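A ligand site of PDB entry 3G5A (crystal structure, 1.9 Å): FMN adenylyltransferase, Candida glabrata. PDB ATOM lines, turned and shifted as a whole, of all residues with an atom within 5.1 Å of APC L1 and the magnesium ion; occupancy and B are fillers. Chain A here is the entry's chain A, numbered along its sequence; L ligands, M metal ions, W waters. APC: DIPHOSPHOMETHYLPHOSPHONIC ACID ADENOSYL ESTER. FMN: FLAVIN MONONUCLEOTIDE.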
ATOM      1  N   SER A  64      14.688  13.062   2.995  1.00  0.00           N
ATOM      2  CA  SER A  64      14.772  14.071   4.082  1.00  0.00           C
ATOM      3  C   SER A  64      13.990  15.356   3.709  1.00  0.00           C
ATOM      4  O   SER A  64      14.267  16.025   2.712  1.00  0.00           O
ATOM      5  CB  SER A  64      16.221  14.349   4.513  1.00  0.00           C
ATOM      6  OG  SER A  64      16.913  15.096   3.540  1.00  0.00           O
ATOM      7  N   TYR A  65      13.006  15.676   4.519  1.00  0.00           N
ATOM      8  CA  TYR A  65      12.086  16.732   4.189  1.00  0.00           C
ATOM      9  C   TYR A  65      11.790  17.622   5.380  1.00  0.00           C
ATOM     10  O   TYR A  65      11.340  17.147   6.413  1.00  0.00           O
ATOM     11  CB  TYR A  65      10.766  16.129   3.694  1.00  0.00           C
ATOM     12  CG  TYR A  65       9.729  17.147   3.188  1.00  0.00           C
ATOM     13  CD1 TYR A  65       9.885  17.782   1.954  1.00  0.00           C
ATOM     14  CD2 TYR A  65       8.583  17.454   3.950  1.00  0.00           C
ATOM     15  CE1 TYR A  65       8.953  18.704   1.485  1.00  0.00           C
ATOM     16  CE2 TYR A  65       7.615  18.371   3.473  1.00  0.00           C
ATOM     17  CZ  TYR A  65       7.820  18.991   2.241  1.00  0.00           C
ATOM     18  OH  TYR A  65       6.909  19.885   1.747  1.00  0.00           O
ATOM     19  N   ASN A  66      11.988  18.925   5.203  1.00  0.00           N
ATOM     20  CA  ASN A  66      11.515  19.855   6.204  1.00  0.00           C
ATOM     21  C   ASN A  66      10.703  21.028   5.639  1.00  0.00           C
ATOM     22  O   ASN A  66      10.726  22.093   6.217  1.00  0.00           O
ATOM     23  CB  ASN A  66      12.694  20.379   7.039  1.00  0.00           C
ATOM     24  CG  ASN A  66      13.648  21.220   6.231  1.00  0.00           C
ATOM     25  OD1 ASN A  66      13.495  21.425   5.005  1.00  0.00           O
ATOM     26  ND2 ASN A  66      14.634  21.743   6.925  1.00  0.00           N
ATOM     27  N   GLY A  67      10.036  20.837   4.497  1.00  0.00           N
ATOM     28  CA  GLY A  67       9.057  21.838   4.004  1.00  0.00           C
ATOM     29  C   GLY A  67       9.652  23.076   3.339  1.00  0.00           C
ATOM     30  O   GLY A  67       8.905  23.916   2.854  1.00  0.00           O
ATOM     31  N   GLY A  68      10.997  23.169   3.337  1.00  0.00           N
ATOM     32  CA  GLY A  68      11.726  24.275   2.665  1.00  0.00           C
ATOM     33  C   GLY A  68      11.628  24.232   1.138  1.00  0.00           C
ATOM     34  O   GLY A  68      11.315  23.198   0.555  1.00  0.00           O
ATOM     35  N   LYS A  69      11.871  25.364   0.484  1.00  0.00           N
ATOM     36  CA  LYS A  69      11.754  25.450  -0.964  1.00  0.00           C
ATOM     37  C   LYS A  69      12.662  24.387  -1.649  1.00  0.00           C
ATOM     38  O   LYS A  69      12.295  23.801  -2.659  1.00  0.00           O
ATOM     39  CB  LYS A  69      12.113  26.879  -1.419  1.00  0.00           C
ATOM     40  CG  LYS A  69      13.654  27.231  -1.195  1.00  0.00           C
ATOM     41  CD  LYS A  69      13.948  28.730  -1.276  1.00  0.00           C
ATOM     42  CE  LYS A  69      15.473  28.987  -1.299  1.00  0.00           C
ATOM     43  NZ  LYS A  69      16.206  28.455  -0.118  1.00  0.00           N
ATOM     44  N   ASP A  70      13.862  24.153  -1.103  1.00  0.00           N
ATOM     45  CA  ASP A  70      14.797  23.292  -1.794  1.00  0.00           C
ATOM     46  C   ASP A  70      14.424  21.811  -1.727  1.00  0.00           C
ATOM     47  O   ASP A  70      14.421  21.094  -2.745  1.00  0.00           O
ATOM     48  CB  ASP A  70      16.214  23.546  -1.278  1.00  0.00           C
ATOM     49  CG  ASP A  70      16.610  25.017  -1.395  1.00  0.00           C
ATOM     50  OD1 ASP A  70      16.766  25.523  -2.514  1.00  0.00           O
ATOM     51  OD2 ASP A  70      16.705  25.677  -0.356  1.00  0.00           O
ATOM     52  N   CYS A  71      14.089  21.324  -0.539  1.00  0.00           N
ATOM     53  CA  CYS A  71      13.594  19.952  -0.490  1.00  0.00           C
ATOM     54  C   CYS A  71      12.258  19.832  -1.235  1.00  0.00           C
ATOM     55  O   CYS A  71      11.985  18.794  -1.787  1.00  0.00           O
ATOM     56  CB  CYS A  71      13.516  19.369   0.938  1.00  0.00           C
ATOM     57  SG  CYS A  71      12.399  20.191   2.013  1.00  0.00           S
ATOM     58  N   GLN A  72      11.432  20.887  -1.230  1.00  0.00           N
ATOM     59  CA  GLN A  72      10.161  20.843  -1.989  1.00  0.00           C
ATOM     60  C   GLN A  72      10.393  20.737  -3.506  1.00  0.00           C
ATOM     61  O   GLN A  72       9.807  19.869  -4.128  1.00  0.00           O
ATOM     62  CB  GLN A  72       9.236  22.026  -1.651  1.00  0.00           C
ATOM     63  CG  GLN A  72       7.855  21.910  -2.376  1.00  0.00           C
ATOM     64  CD  GLN A  72       6.857  23.038  -2.049  1.00  0.00           C
ATOM     65  OE1 GLN A  72       7.215  24.070  -1.466  1.00  0.00           O
ATOM     66  NE2 GLN A  72       5.584  22.821  -2.441  1.00  0.00           N
ATOM     67  N   VAL A 110      11.616  11.551   6.150  1.00  0.00           N
ATOM     68  CA  VAL A 110      12.123  11.800   7.505  1.00  0.00           C
ATOM     69  C   VAL A 110      12.273  13.303   7.770  1.00  0.00           C
ATOM     70  O   VAL A 110      12.848  14.030   6.964  1.00  0.00           O
ATOM     71  CB  VAL A 110      13.450  11.029   7.772  1.00  0.00           C
ATOM     72  CG1 VAL A 110      14.484  11.289   6.683  1.00  0.00           C
ATOM     73  CG2 VAL A 110      14.026  11.332   9.188  1.00  0.00           C
ATOM     74  N   PHE A 111      11.739  13.736   8.903  1.00  0.00           N
ATOM     75  CA  PHE A 111      11.814  15.120   9.301  1.00  0.00           C
ATOM     76  C   PHE A 111      12.355  15.167  10.723  1.00  0.00           C
ATOM     77  O   PHE A 111      11.776  14.578  11.636  1.00  0.00           O
ATOM     78  CB  PHE A 111      10.444  15.811   9.161  1.00  0.00           C
ATOM     79  CG  PHE A 111      10.319  17.136   9.896  1.00  0.00           C
ATOM     80  CD1 PHE A 111      11.247  18.158   9.676  1.00  0.00           C
ATOM     81  CD2 PHE A 111       9.256  17.362  10.775  1.00  0.00           C
ATOM     82  CE1 PHE A 111      11.138  19.412  10.322  1.00  0.00           C
ATOM     83  CE2 PHE A 111       9.129  18.606  11.443  1.00  0.00           C
ATOM     84  CZ  PHE A 111      10.092  19.631  11.222  1.00  0.00           C
ATOM     85  N   ILE A 112      13.455  15.857  10.908  1.00  0.00           N
ATOM     86  CA  ILE A 112      13.983  16.057  12.252  1.00  0.00           C
ATOM     87  C   ILE A 112      13.428  17.360  12.840  1.00  0.00           C
ATOM     88  O   ILE A 112      13.851  18.434  12.470  1.00  0.00           O
ATOM     89  CB  ILE A 112      15.543  16.032  12.310  1.00  0.00           C
ATOM     90  CG1 ILE A 112      16.094  14.752  11.646  1.00  0.00           C
ATOM     91  CG2 ILE A 112      16.038  16.173  13.797  1.00  0.00           C
ATOM     92  CD1 ILE A 112      15.354  13.425  12.023  1.00  0.00           C
ATOM     93  N   ASP A 113      12.465  17.223  13.744  1.00  0.00           N
ATOM     94  CA  ASP A 113      11.749  18.384  14.277  1.00  0.00           C
ATOM     95  C   ASP A 113      12.600  19.023  15.387  1.00  0.00           C
ATOM     96  O   ASP A 113      13.396  18.327  16.049  1.00  0.00           O
ATOM     97  CB  ASP A 113      10.421  17.886  14.831  1.00  0.00           C
ATOM     98  CG  ASP A 113       9.396  19.007  15.038  1.00  0.00           C
ATOM     99  OD1 ASP A 113       9.652  20.174  14.672  1.00  0.00           O
ATOM    100  OD2 ASP A 113       8.330  18.699  15.587  1.00  0.00           O
ATOM    101  N   HIS A 114      12.430  20.323  15.599  1.00  0.00           N
ATOM    102  CA  HIS A 114      13.145  21.040  16.664  1.00  0.00           C
ATOM    103  C   HIS A 114      12.202  21.978  17.382  1.00  0.00           C
ATOM    104  O   HIS A 114      11.173  22.379  16.806  1.00  0.00           O
ATOM    105  CB  HIS A 114      14.342  21.806  16.113  1.00  0.00           C
ATOM    106  CG  HIS A 114      15.371  20.935  15.454  1.00  0.00           C
ATOM    107  ND1 HIS A 114      15.407  20.744  14.086  1.00  0.00           N
ATOM    108  CD2 HIS A 114      16.367  20.184  15.973  1.00  0.00           C
ATOM    109  CE1 HIS A 114      16.398  19.927  13.793  1.00  0.00           C
ATOM    110  NE2 HIS A 114      16.998  19.562  14.914  1.00  0.00           N
ATOM    111  N   MET A 147      21.643  16.467  14.959  1.00  0.00           N
ATOM    112  CA  MET A 147      21.025  15.823  13.768  1.00  0.00           C
ATOM    113  C   MET A 147      21.526  14.397  13.537  1.00  0.00           C
ATOM    114  O   MET A 147      20.738  13.503  13.236  1.00  0.00           O
ATOM    115  CB  MET A 147      21.281  16.665  12.516  1.00  0.00           C
ATOM    116  CG  MET A 147      20.535  17.983  12.553  1.00  0.00           C
ATOM    117  SD  MET A 147      18.836  17.704  12.124  1.00  0.00           S
ATOM    118  CE  MET A 147      19.056  17.677  10.318  1.00  0.00           C
ATOM    119  N   PHE A 151      19.326  11.020  13.490  1.00  0.00           N
ATOM    120  CA  PHE A 151      19.383  10.096  12.347  1.00  0.00           C
ATOM    121  C   PHE A 151      19.862   8.693  12.743  1.00  0.00           C
ATOM    122  O   PHE A 151      19.465   7.708  12.111  1.00  0.00           O
ATOM    123  CB  PHE A 151      20.186  10.675  11.171  1.00  0.00           C
ATOM    124  CG  PHE A 151      19.351  11.551  10.243  1.00  0.00           C
ATOM    125  CD1 PHE A 151      18.507  10.969   9.275  1.00  0.00           C
ATOM    126  CD2 PHE A 151      19.390  12.926  10.358  1.00  0.00           C
ATOM    127  CE1 PHE A 151      17.723  11.767   8.452  1.00  0.00           C
ATOM    128  CE2 PHE A 151      18.607  13.746   9.531  1.00  0.00           C
ATOM    129  CZ  PHE A 151      17.758  13.159   8.585  1.00  0.00           C
ATOM    130  N   VAL A 165      17.859  11.054   0.663  1.00  0.00           N
ATOM    131  CA  VAL A 165      17.811  12.193  -0.255  1.00  0.00           C
ATOM    132  C   VAL A 165      17.780  13.528   0.498  1.00  0.00           C
ATOM    133  O   VAL A 165      16.967  13.738   1.409  1.00  0.00           O
ATOM    134  CB  VAL A 165      16.600  12.085  -1.186  1.00  0.00           C
ATOM    135  CG1 VAL A 165      16.601  13.185  -2.240  1.00  0.00           C
ATOM    136  CG2 VAL A 165      16.534  10.660  -1.780  1.00  0.00           C
ATOM    137  N   ILE A 166      18.668  14.424   0.107  1.00  0.00           N
ATOM    138  CA  ILE A 166      18.873  15.703   0.819  1.00  0.00           C
ATOM    139  C   ILE A 166      18.902  16.865  -0.185  1.00  0.00           C
ATOM    140  O   ILE A 166      19.603  16.790  -1.201  1.00  0.00           O
ATOM    141  CB  ILE A 166      20.219  15.719   1.593  1.00  0.00           C
ATOM    142  CG1 ILE A 166      20.375  14.472   2.439  1.00  0.00           C
ATOM    143  CG2 ILE A 166      20.380  17.027   2.462  1.00  0.00           C
ATOM    144  CD1 ILE A 166      21.820  14.170   2.782  1.00  0.00           C
ATOM    145  N   GLY A 167      18.156  17.926   0.092  1.00  0.00           N
ATOM    146  CA  GLY A 167      18.059  19.053  -0.854  1.00  0.00           C
ATOM    147  C   GLY A 167      19.083  20.183  -0.638  1.00  0.00           C
ATOM    148  O   GLY A 167      18.767  21.368  -0.730  1.00  0.00           O
ATOM    149  N   ILE A 168      20.319  19.803  -0.340  1.00  0.00           N
ATOM    150  CA  ILE A 168      21.422  20.733  -0.158  1.00  0.00           C
ATOM    151  C   ILE A 168      21.929  21.170  -1.541  1.00  0.00           C
ATOM    152  O   ILE A 168      21.854  20.431  -2.514  1.00  0.00           O
ATOM    153  CB  ILE A 168      22.536  20.059   0.752  1.00  0.00           C
ATOM    154  CG1 ILE A 168      23.711  21.006   0.991  1.00  0.00           C
ATOM    155  CG2 ILE A 168      23.023  18.753   0.134  1.00  0.00           C
ATOM    156  CD1 ILE A 168      24.322  20.881   2.384  1.00  0.00           C
ATOM    157  N   ARG A 169      22.403  22.408  -1.626  1.00  0.00           N
ATOM    158  CA  ARG A 169      22.967  22.958  -2.857  1.00  0.00           C
ATOM    159  C   ARG A 169      24.381  23.400  -2.578  1.00  0.00           C
ATOM    160  O   ARG A 169      24.728  23.655  -1.416  1.00  0.00           O
ATOM    161  CB  ARG A 169      22.115  24.132  -3.352  1.00  0.00           C
ATOM    162  CG  ARG A 169      20.655  23.670  -3.495  1.00  0.00           C
ATOM    163  CD  ARG A 169      19.844  24.589  -4.309  1.00  0.00           C
ATOM    164  NE  ARG A 169      19.303  25.634  -3.511  1.00  0.00           N
ATOM    165  CZ  ARG A 169      19.670  26.915  -3.553  1.00  0.00           C
ATOM    166  NH1 ARG A 169      20.650  27.318  -4.342  1.00  0.00           N
ATOM    167  NH2 ARG A 169      19.065  27.771  -2.781  1.00  0.00           N
ATOM    168  N   ASP A 172      25.055  26.416  -0.385  1.00  0.00           N
ATOM    169  CA  ASP A 172      24.732  26.316   1.057  1.00  0.00           C
ATOM    170  C   ASP A 172      26.021  26.208   1.864  1.00  0.00           C
ATOM    171  O   ASP A 172      27.043  25.812   1.312  1.00  0.00           O
ATOM    172  CB  ASP A 172      23.835  25.101   1.323  1.00  0.00           C
ATOM    173  CG  ASP A 172      22.470  25.217   0.647  1.00  0.00           C
ATOM    174  OD1 ASP A 172      22.094  26.330   0.172  1.00  0.00           O
ATOM    175  OD2 ASP A 172      21.780  24.188   0.594  1.00  0.00           O
ATOM    176  N   TYR A 220       7.783  32.493   2.732  1.00  0.00           N
ATOM    177  CA  TYR A 220       8.416  33.070   1.536  1.00  0.00           C
ATOM    178  C   TYR A 220       7.664  34.317   0.987  1.00  0.00           C
ATOM    179  O   TYR A 220       8.278  35.329   0.658  1.00  0.00           O
ATOM    180  CB  TYR A 220       8.666  32.006   0.458  1.00  0.00           C
ATOM    181  CG  TYR A 220       9.615  30.902   0.929  1.00  0.00           C
ATOM    182  CD1 TYR A 220      10.876  31.206   1.448  1.00  0.00           C
ATOM    183  CD2 TYR A 220       9.273  29.556   0.820  1.00  0.00           C
ATOM    184  CE1 TYR A 220      11.757  30.200   1.871  1.00  0.00           C
ATOM    185  CE2 TYR A 220      10.140  28.546   1.244  1.00  0.00           C
ATOM    186  CZ  TYR A 220      11.385  28.882   1.757  1.00  0.00           C
ATOM    187  OH  TYR A 220      12.230  27.893   2.167  1.00  0.00           O
ATOM    188  N   THR A 225      13.807  34.374   2.719  1.00  0.00           N
ATOM    189  CA  THR A 225      14.467  33.688   1.590  1.00  0.00           C
ATOM    190  C   THR A 225      15.211  32.464   2.115  1.00  0.00           C
ATOM    191  O   THR A 225      15.640  31.577   1.339  1.00  0.00           O
ATOM    192  CB  THR A 225      15.495  34.623   0.887  1.00  0.00           C
ATOM    193  OG1 THR A 225      16.421  35.102   1.853  1.00  0.00           O
ATOM    194  CG2 THR A 225      14.805  35.846   0.261  1.00  0.00           C
ATOM    195  N   SER A 226      15.386  32.423   3.422  1.00  0.00           N
ATOM    196  CA  SER A 226      16.062  31.308   4.080  1.00  0.00           C
ATOM    197  C   SER A 226      15.380  31.023   5.395  1.00  0.00           C
ATOM    198  O   SER A 226      15.081  31.943   6.174  1.00  0.00           O
ATOM    199  CB  SER A 226      17.571  31.630   4.238  1.00  0.00           C
ATOM    200  OG  SER A 226      18.279  30.708   5.043  1.00  0.00           O
ATOM    201  N   LEU A 227      15.107  29.746   5.679  1.00  0.00           N
ATOM    202  CA  LEU A 227      14.383  29.406   6.883  1.00  0.00           C
ATOM    203  C   LEU A 227      15.296  28.732   7.886  1.00  0.00           C
ATOM    204  O   LEU A 227      15.594  27.545   7.786  1.00  0.00           O
ATOM    205  CB  LEU A 227      13.118  28.576   6.572  1.00  0.00           C
ATOM    206  CG  LEU A 227      12.063  29.134   5.581  1.00  0.00           C
ATOM    207  CD1 LEU A 227      10.852  28.191   5.514  1.00  0.00           C
ATOM    208  CD2 LEU A 227      11.593  30.571   5.901  1.00  0.00           C
ATOM    209  N   GLU A 300      21.326  34.928   0.278  1.00  0.00           N
ATOM    210  CA  GLU A 300      20.168  34.091   0.628  1.00  0.00           C
ATOM    211  C   GLU A 300      19.985  34.034   2.154  1.00  0.00           C
ATOM    212  O   GLU A 300      18.846  33.989   2.655  1.00  0.00           O
ATOM    213  CB  GLU A 300      20.304  32.704   0.026  1.00  0.00           C
ATOM    214  CG  GLU A 300      19.120  31.768   0.324  1.00  0.00           C
ATOM    215  CD  GLU A 300      19.230  30.406  -0.344  1.00  0.00           C
ATOM    216  OE1 GLU A 300      19.809  30.301  -1.445  1.00  0.00           O
ATOM    217  OE2 GLU A 300      18.724  29.428   0.243  1.00  0.00           O
ATOM    218  N   ARG A 301      21.107  34.026   2.882  1.00  0.00           N
ATOM    219  CA  ARG A 301      21.067  33.951   4.360  1.00  0.00           C
ATOM    220  C   ARG A 301      21.201  35.269   5.075  1.00  0.00           C
ATOM    221  O   ARG A 301      21.383  35.269   6.304  1.00  0.00           O
ATOM    222  CB  ARG A 301      22.071  32.918   4.879  1.00  0.00           C
ATOM    223  CG  ARG A 301      21.647  31.511   4.445  1.00  0.00           C
ATOM    224  CD  ARG A 301      22.716  30.496   4.503  1.00  0.00           C
ATOM    225  NE  ARG A 301      22.273  29.337   3.730  1.00  0.00           N
ATOM    226  CZ  ARG A 301      22.384  29.229   2.408  1.00  0.00           C
ATOM    227  NH1 ARG A 301      21.908  28.168   1.820  1.00  0.00           N
ATOM    228  NH2 ARG A 301      22.992  30.177   1.653  1.00  0.00           N
HETATM  229  PG  APC L   1      15.627  26.978   2.928  1.00  0.00           P
HETATM  230  O1G APC L   1      15.671  26.852   4.445  1.00  0.00           O
HETATM  231  O2G APC L   1      14.718  28.068   2.439  1.00  0.00           O
HETATM  232  O3G APC L   1      16.997  27.096   2.321  1.00  0.00           O
HETATM  233  PB  APC L   1      15.442  24.055   2.506  1.00  0.00           P
HETATM  234  O1B APC L   1      14.504  23.095   1.841  1.00  0.00           O
HETATM  235  O2B APC L   1      16.899  23.992   2.114  1.00  0.00           O
HETATM  236  O3B APC L   1      14.940  25.584   2.352  1.00  0.00           O
HETATM  237  PA  APC L   1      17.031  23.486   5.154  1.00  0.00           P
HETATM  238  O1A APC L   1      16.736  23.401   6.634  1.00  0.00           O
HETATM  239  O2A APC L   1      17.879  24.667   4.742  1.00  0.00           O
HETATM  240  C3A APC L   1      15.430  23.615   4.283  1.00  0.00           C
HETATM  241  O5' APC L   1      17.884  22.117   4.779  1.00  0.00           O
HETATM  242  C5' APC L   1      18.584  21.727   3.556  1.00  0.00           C
HETATM  243  C4' APC L   1      18.377  20.242   3.156  1.00  0.00           C
HETATM  244  O4' APC L   1      18.690  19.426   4.300  1.00  0.00           O
HETATM  245  C3' APC L   1      16.853  20.155   3.037  1.00  0.00           C
HETATM  246  O3' APC L   1      16.385  20.282   1.704  1.00  0.00           O
HETATM  247  C2' APC L   1      16.501  18.805   3.629  1.00  0.00           C
HETATM  248  O2' APC L   1      16.662  17.760   2.640  1.00  0.00           O
HETATM  249  C1' APC L   1      17.598  18.588   4.650  1.00  0.00           C
HETATM  250  N9  APC L   1      17.179  18.978   6.024  1.00  0.00           N
HETATM  251  C8  APC L   1      17.615  20.065   6.698  1.00  0.00           C
HETATM  252  N7  APC L   1      17.042  20.096   7.915  1.00  0.00           N
HETATM  253  C5  APC L   1      16.255  19.000   8.027  1.00  0.00           C
HETATM  254  C6  APC L   1      15.398  18.523   9.032  1.00  0.00           C
HETATM  255  N6  APC L   1      15.246  19.151  10.230  1.00  0.00           N
HETATM  256  N1  APC L   1      14.718  17.374   8.797  1.00  0.00           N
HETATM  257  C2  APC L   1      14.819  16.699   7.628  1.00  0.00           C
HETATM  258  N3  APC L   1      15.609  17.159   6.647  1.00  0.00           N
HETATM  259  C4  APC L   1      16.324  18.299   6.812  1.00  0.00           C
HETATM  260  N1  FMN L   2      26.896  17.023   7.669  1.00  0.00           N
HETATM  261  C2  FMN L   2      28.202  16.562   7.737  1.00  0.00           C
HETATM  262  O2  FMN L   2      29.151  17.315   8.063  1.00  0.00           O
HETATM  263  N3  FMN L   2      28.424  15.221   7.451  1.00  0.00           N
HETATM  264  C4  FMN L   2      27.408  14.365   7.124  1.00  0.00           C
HETATM  265  O4  FMN L   2      27.680  13.165   6.995  1.00  0.00           O
HETATM  266  C4A FMN L   2      26.104  14.845   7.032  1.00  0.00           C
HETATM  267  N5  FMN L   2      25.067  14.007   6.671  1.00  0.00           N
HETATM  268  C5A FMN L   2      23.754  14.515   6.584  1.00  0.00           C
HETATM  269  C6  FMN L   2      22.686  13.681   6.212  1.00  0.00           C
HETATM  270  C7  FMN L   2      21.367  14.162   6.150  1.00  0.00           C
HETATM  271  C7M FMN L   2      20.245  13.180   6.009  1.00  0.00           C
HETATM  272  C8  FMN L   2      21.124  15.526   6.432  1.00  0.00           C
HETATM  273  C8M FMN L   2      19.747  16.146   6.325  1.00  0.00           C
HETATM  274  C9  FMN L   2      22.183  16.361   6.783  1.00  0.00           C
HETATM  275  C9A FMN L   2      23.505  15.869   6.857  1.00  0.00           C
HETATM  276  N10 FMN L   2      24.552  16.722   7.205  1.00  0.00           N
HETATM  277  C10 FMN L   2      25.846  16.203   7.304  1.00  0.00           C
HETATM  278  C1' FMN L   2      24.267  18.207   7.394  1.00  0.00           C
HETATM  279  C2' FMN L   2      24.255  18.592   8.879  1.00  0.00           C
HETATM  280  O2' FMN L   2      23.139  17.996   9.531  1.00  0.00           O
HETATM  281  C3' FMN L   2      24.306  20.097   9.235  1.00  0.00           C
HETATM  282  O3' FMN L   2      25.321  20.743   8.493  1.00  0.00           O
HETATM  283  C4' FMN L   2      24.670  20.332  10.715  1.00  0.00           C
HETATM  284  O4' FMN L   2      25.969  19.843  10.931  1.00  0.00           O
HETATM  285  C5' FMN L   2      23.744  19.692  11.761  1.00  0.00           C
HETATM  286  O5' FMN L   2      23.716  20.407  12.983  1.00  0.00           O
HETATM  287  P   FMN L   2      23.847  19.665  14.428  1.00  0.00           P
HETATM  288  O1P FMN L   2      24.227  20.689  15.470  1.00  0.00           O
HETATM  289  O2P FMN L   2      24.970  18.665  14.351  1.00  0.00           O
HETATM  290  O3P FMN L   2      22.599  18.969  14.835  1.00  0.00           O
HETATM  291 MG    MG M   1      18.206  25.523   1.210  1.00  0.00          MG
HETATM  292  O   HOH W   1      16.985  21.551  10.751  1.00  0.00           O
HETATM  293  O   HOH W   2      19.510  26.956   0.263  1.00  0.00           O
HETATM  294  O   HOH W   3      19.370  23.938   0.152  1.00  0.00           O
HETATM  295  O   HOH W   4      19.637  25.441   2.957  1.00  0.00           O
HETATM  296  O   HOH W   5      19.580  21.085   9.869  1.00  0.00           O
HETATM  297  O   HOH W   6      14.158  25.128   7.825  1.00  0.00           O
HETATM  298  O   HOH W   7      21.202  19.683   5.400  1.00  0.00           O
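The magnesium ion is bound by water W2 (2.2 Å), the side-chain carboxylate of Asp 70 (2.2 Å), an oxygen (O2B) of APC L1 (2.2 Å), water W3 (2.2 Å), water W4 (2.3 Å) and an oxygen (O3G) of APC L1 (2.3 Å).
A nitrogen (N6) of APC L1 sits at hydrogen-bond distance from the backbone carbonyl oxygen (O) of Ile 112. ND2 of Asn 66 is in hydrogen-bond range of O1A of APC L1 (2.7 Å). The backbone NH (N) of Cys 71 sits at hydrogen-bond distance from an oxygen (O1B) of APC L1 (3.0 Å). The side-chain hydroxyl (OH) of Tyr 220 sits at hydrogen-bond distance from an oxygen (O2G) of APC L1 (2.5 Å). N of Met 147 is in hydrogen-bond range of O3P of FMN L2 (2.7 Å). The backbone NH (N) of Gly 167 sits at hydrogen-bond distance from an oxygen (O2') of APC L1 (3.0 Å). O2' of APC L1 is in hydrogen-bond range of O of Ser 64 (3.0 Å). An oxygen (O1B) of APC L1 lies within hydrogen-bond range of the backbone NH of Asp 70 (3.2 Å). NZ of Lys 69 sits at hydrogen-bond distance from O2G of APC L1, 3.0 Å away. O1B of APC L1 sits at hydrogen-bond distance from SG of Cys 71 (3.6 Å). N of Leu 227 sits at hydrogen-bond distance from O1G of APC L1, 3.2 Å away. An oxygen (O2') of APC L1 sits at hydrogen-bond distance from the side-chain hydroxyl (OG) of Ser 64, at 2.8 Å. The backbone NH (N) of Ile 112 is in hydrogen-bond range of a nitrogen (N1) of APC L1, 2.9 Å away.
The backbone carbonyl oxygen (O) of Gly 68 is in hydrogen-bond range of the side-chain sulfur (SG) of Cys 71 (3.5 Å). OD2 of Asp 172 is in hydrogen-bond range of N of Arg 169 (2.9 Å). The guanidinium group (NH1) of Arg 301 lies within salt-bridge range of the side-chain carboxylate (OE2) of Glu 300 (3.8 Å). The side-chain sulfur of Cys 71 lies within hydrogen-bond range of the backbone NH of Gly 67, 3.5 Å away. The side-chain sulfur (SG) of Cys 71 sits at hydrogen-bond distance from the side-chain amide oxygen (OD1) of Asn 66, 3.4 Å away. The backbone NH (N) of Gly 68 sits close to the side-chain amide oxygen (OD1) of Asn 66, 3.5 Å away. The side-chain carboxylate (OD1) of Asp 172 lies within salt-bridge range of the guanidinium group (NH1) of Arg 301, 2.5 Å away. The side-chain carboxylate (OD1) of Asp 70 is in salt-bridge range of the guanidinium group (NE) of Arg 169 (2.7 Å).
O1B of APC L1 sits close to O of Gly 68, at 3.4 Å. Tyr 65 touches APC L1. O of Val 110 touches C2 of APC L1, at 3.4 Å. Phe 111 touches APC L1. CE1 of His 114 touches N6 of APC L1, at 3.8 Å. Met 147 touches APC L1 (CE to C5, 3.9 Å). Ile 166 touches APC L1 (CG2 to O4', 3.5 Å). Thr 225 touches APC L1. CA of Ser 226 touches O2G of APC L1 (3.9 Å). OE2 of Glu 300 touches O3G of APC L1, 3.6 Å away. Of the 28 residues printed, 19 come within 4 Å of APC L1. The nearest printed residue that does not touch APC L1 is Ile 168 (4.02 Å).
Water W3 bridges the side-chain carboxylate (OD2) of Asp 172 (2.5 Å) and the backbone carbonyl oxygen (O) of Gly 167 (2.8 Å). Water W4 lies within hydrogen-bond range of an oxygen (O2A) of APC L1 and the side-chain carboxylate (OD2) of Asp 172. Water W2 lies within hydrogen-bond range of the side-chain carboxylate of Glu 300 (2.6 Å), the side-chain carboxylate of Asp 172 (2.7 Å), the guanidinium group of Arg 301 (3.1 Å) and the guanidinium group of Arg 169 (3.2 Å). Water W6 lies within hydrogen-bond range of O of Leu 227 (2.8 Å) and O1A of APC L1 (3.3 Å).
Lys 69 touches the magnesium ion. Asp 172 touches the magnesium ion.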
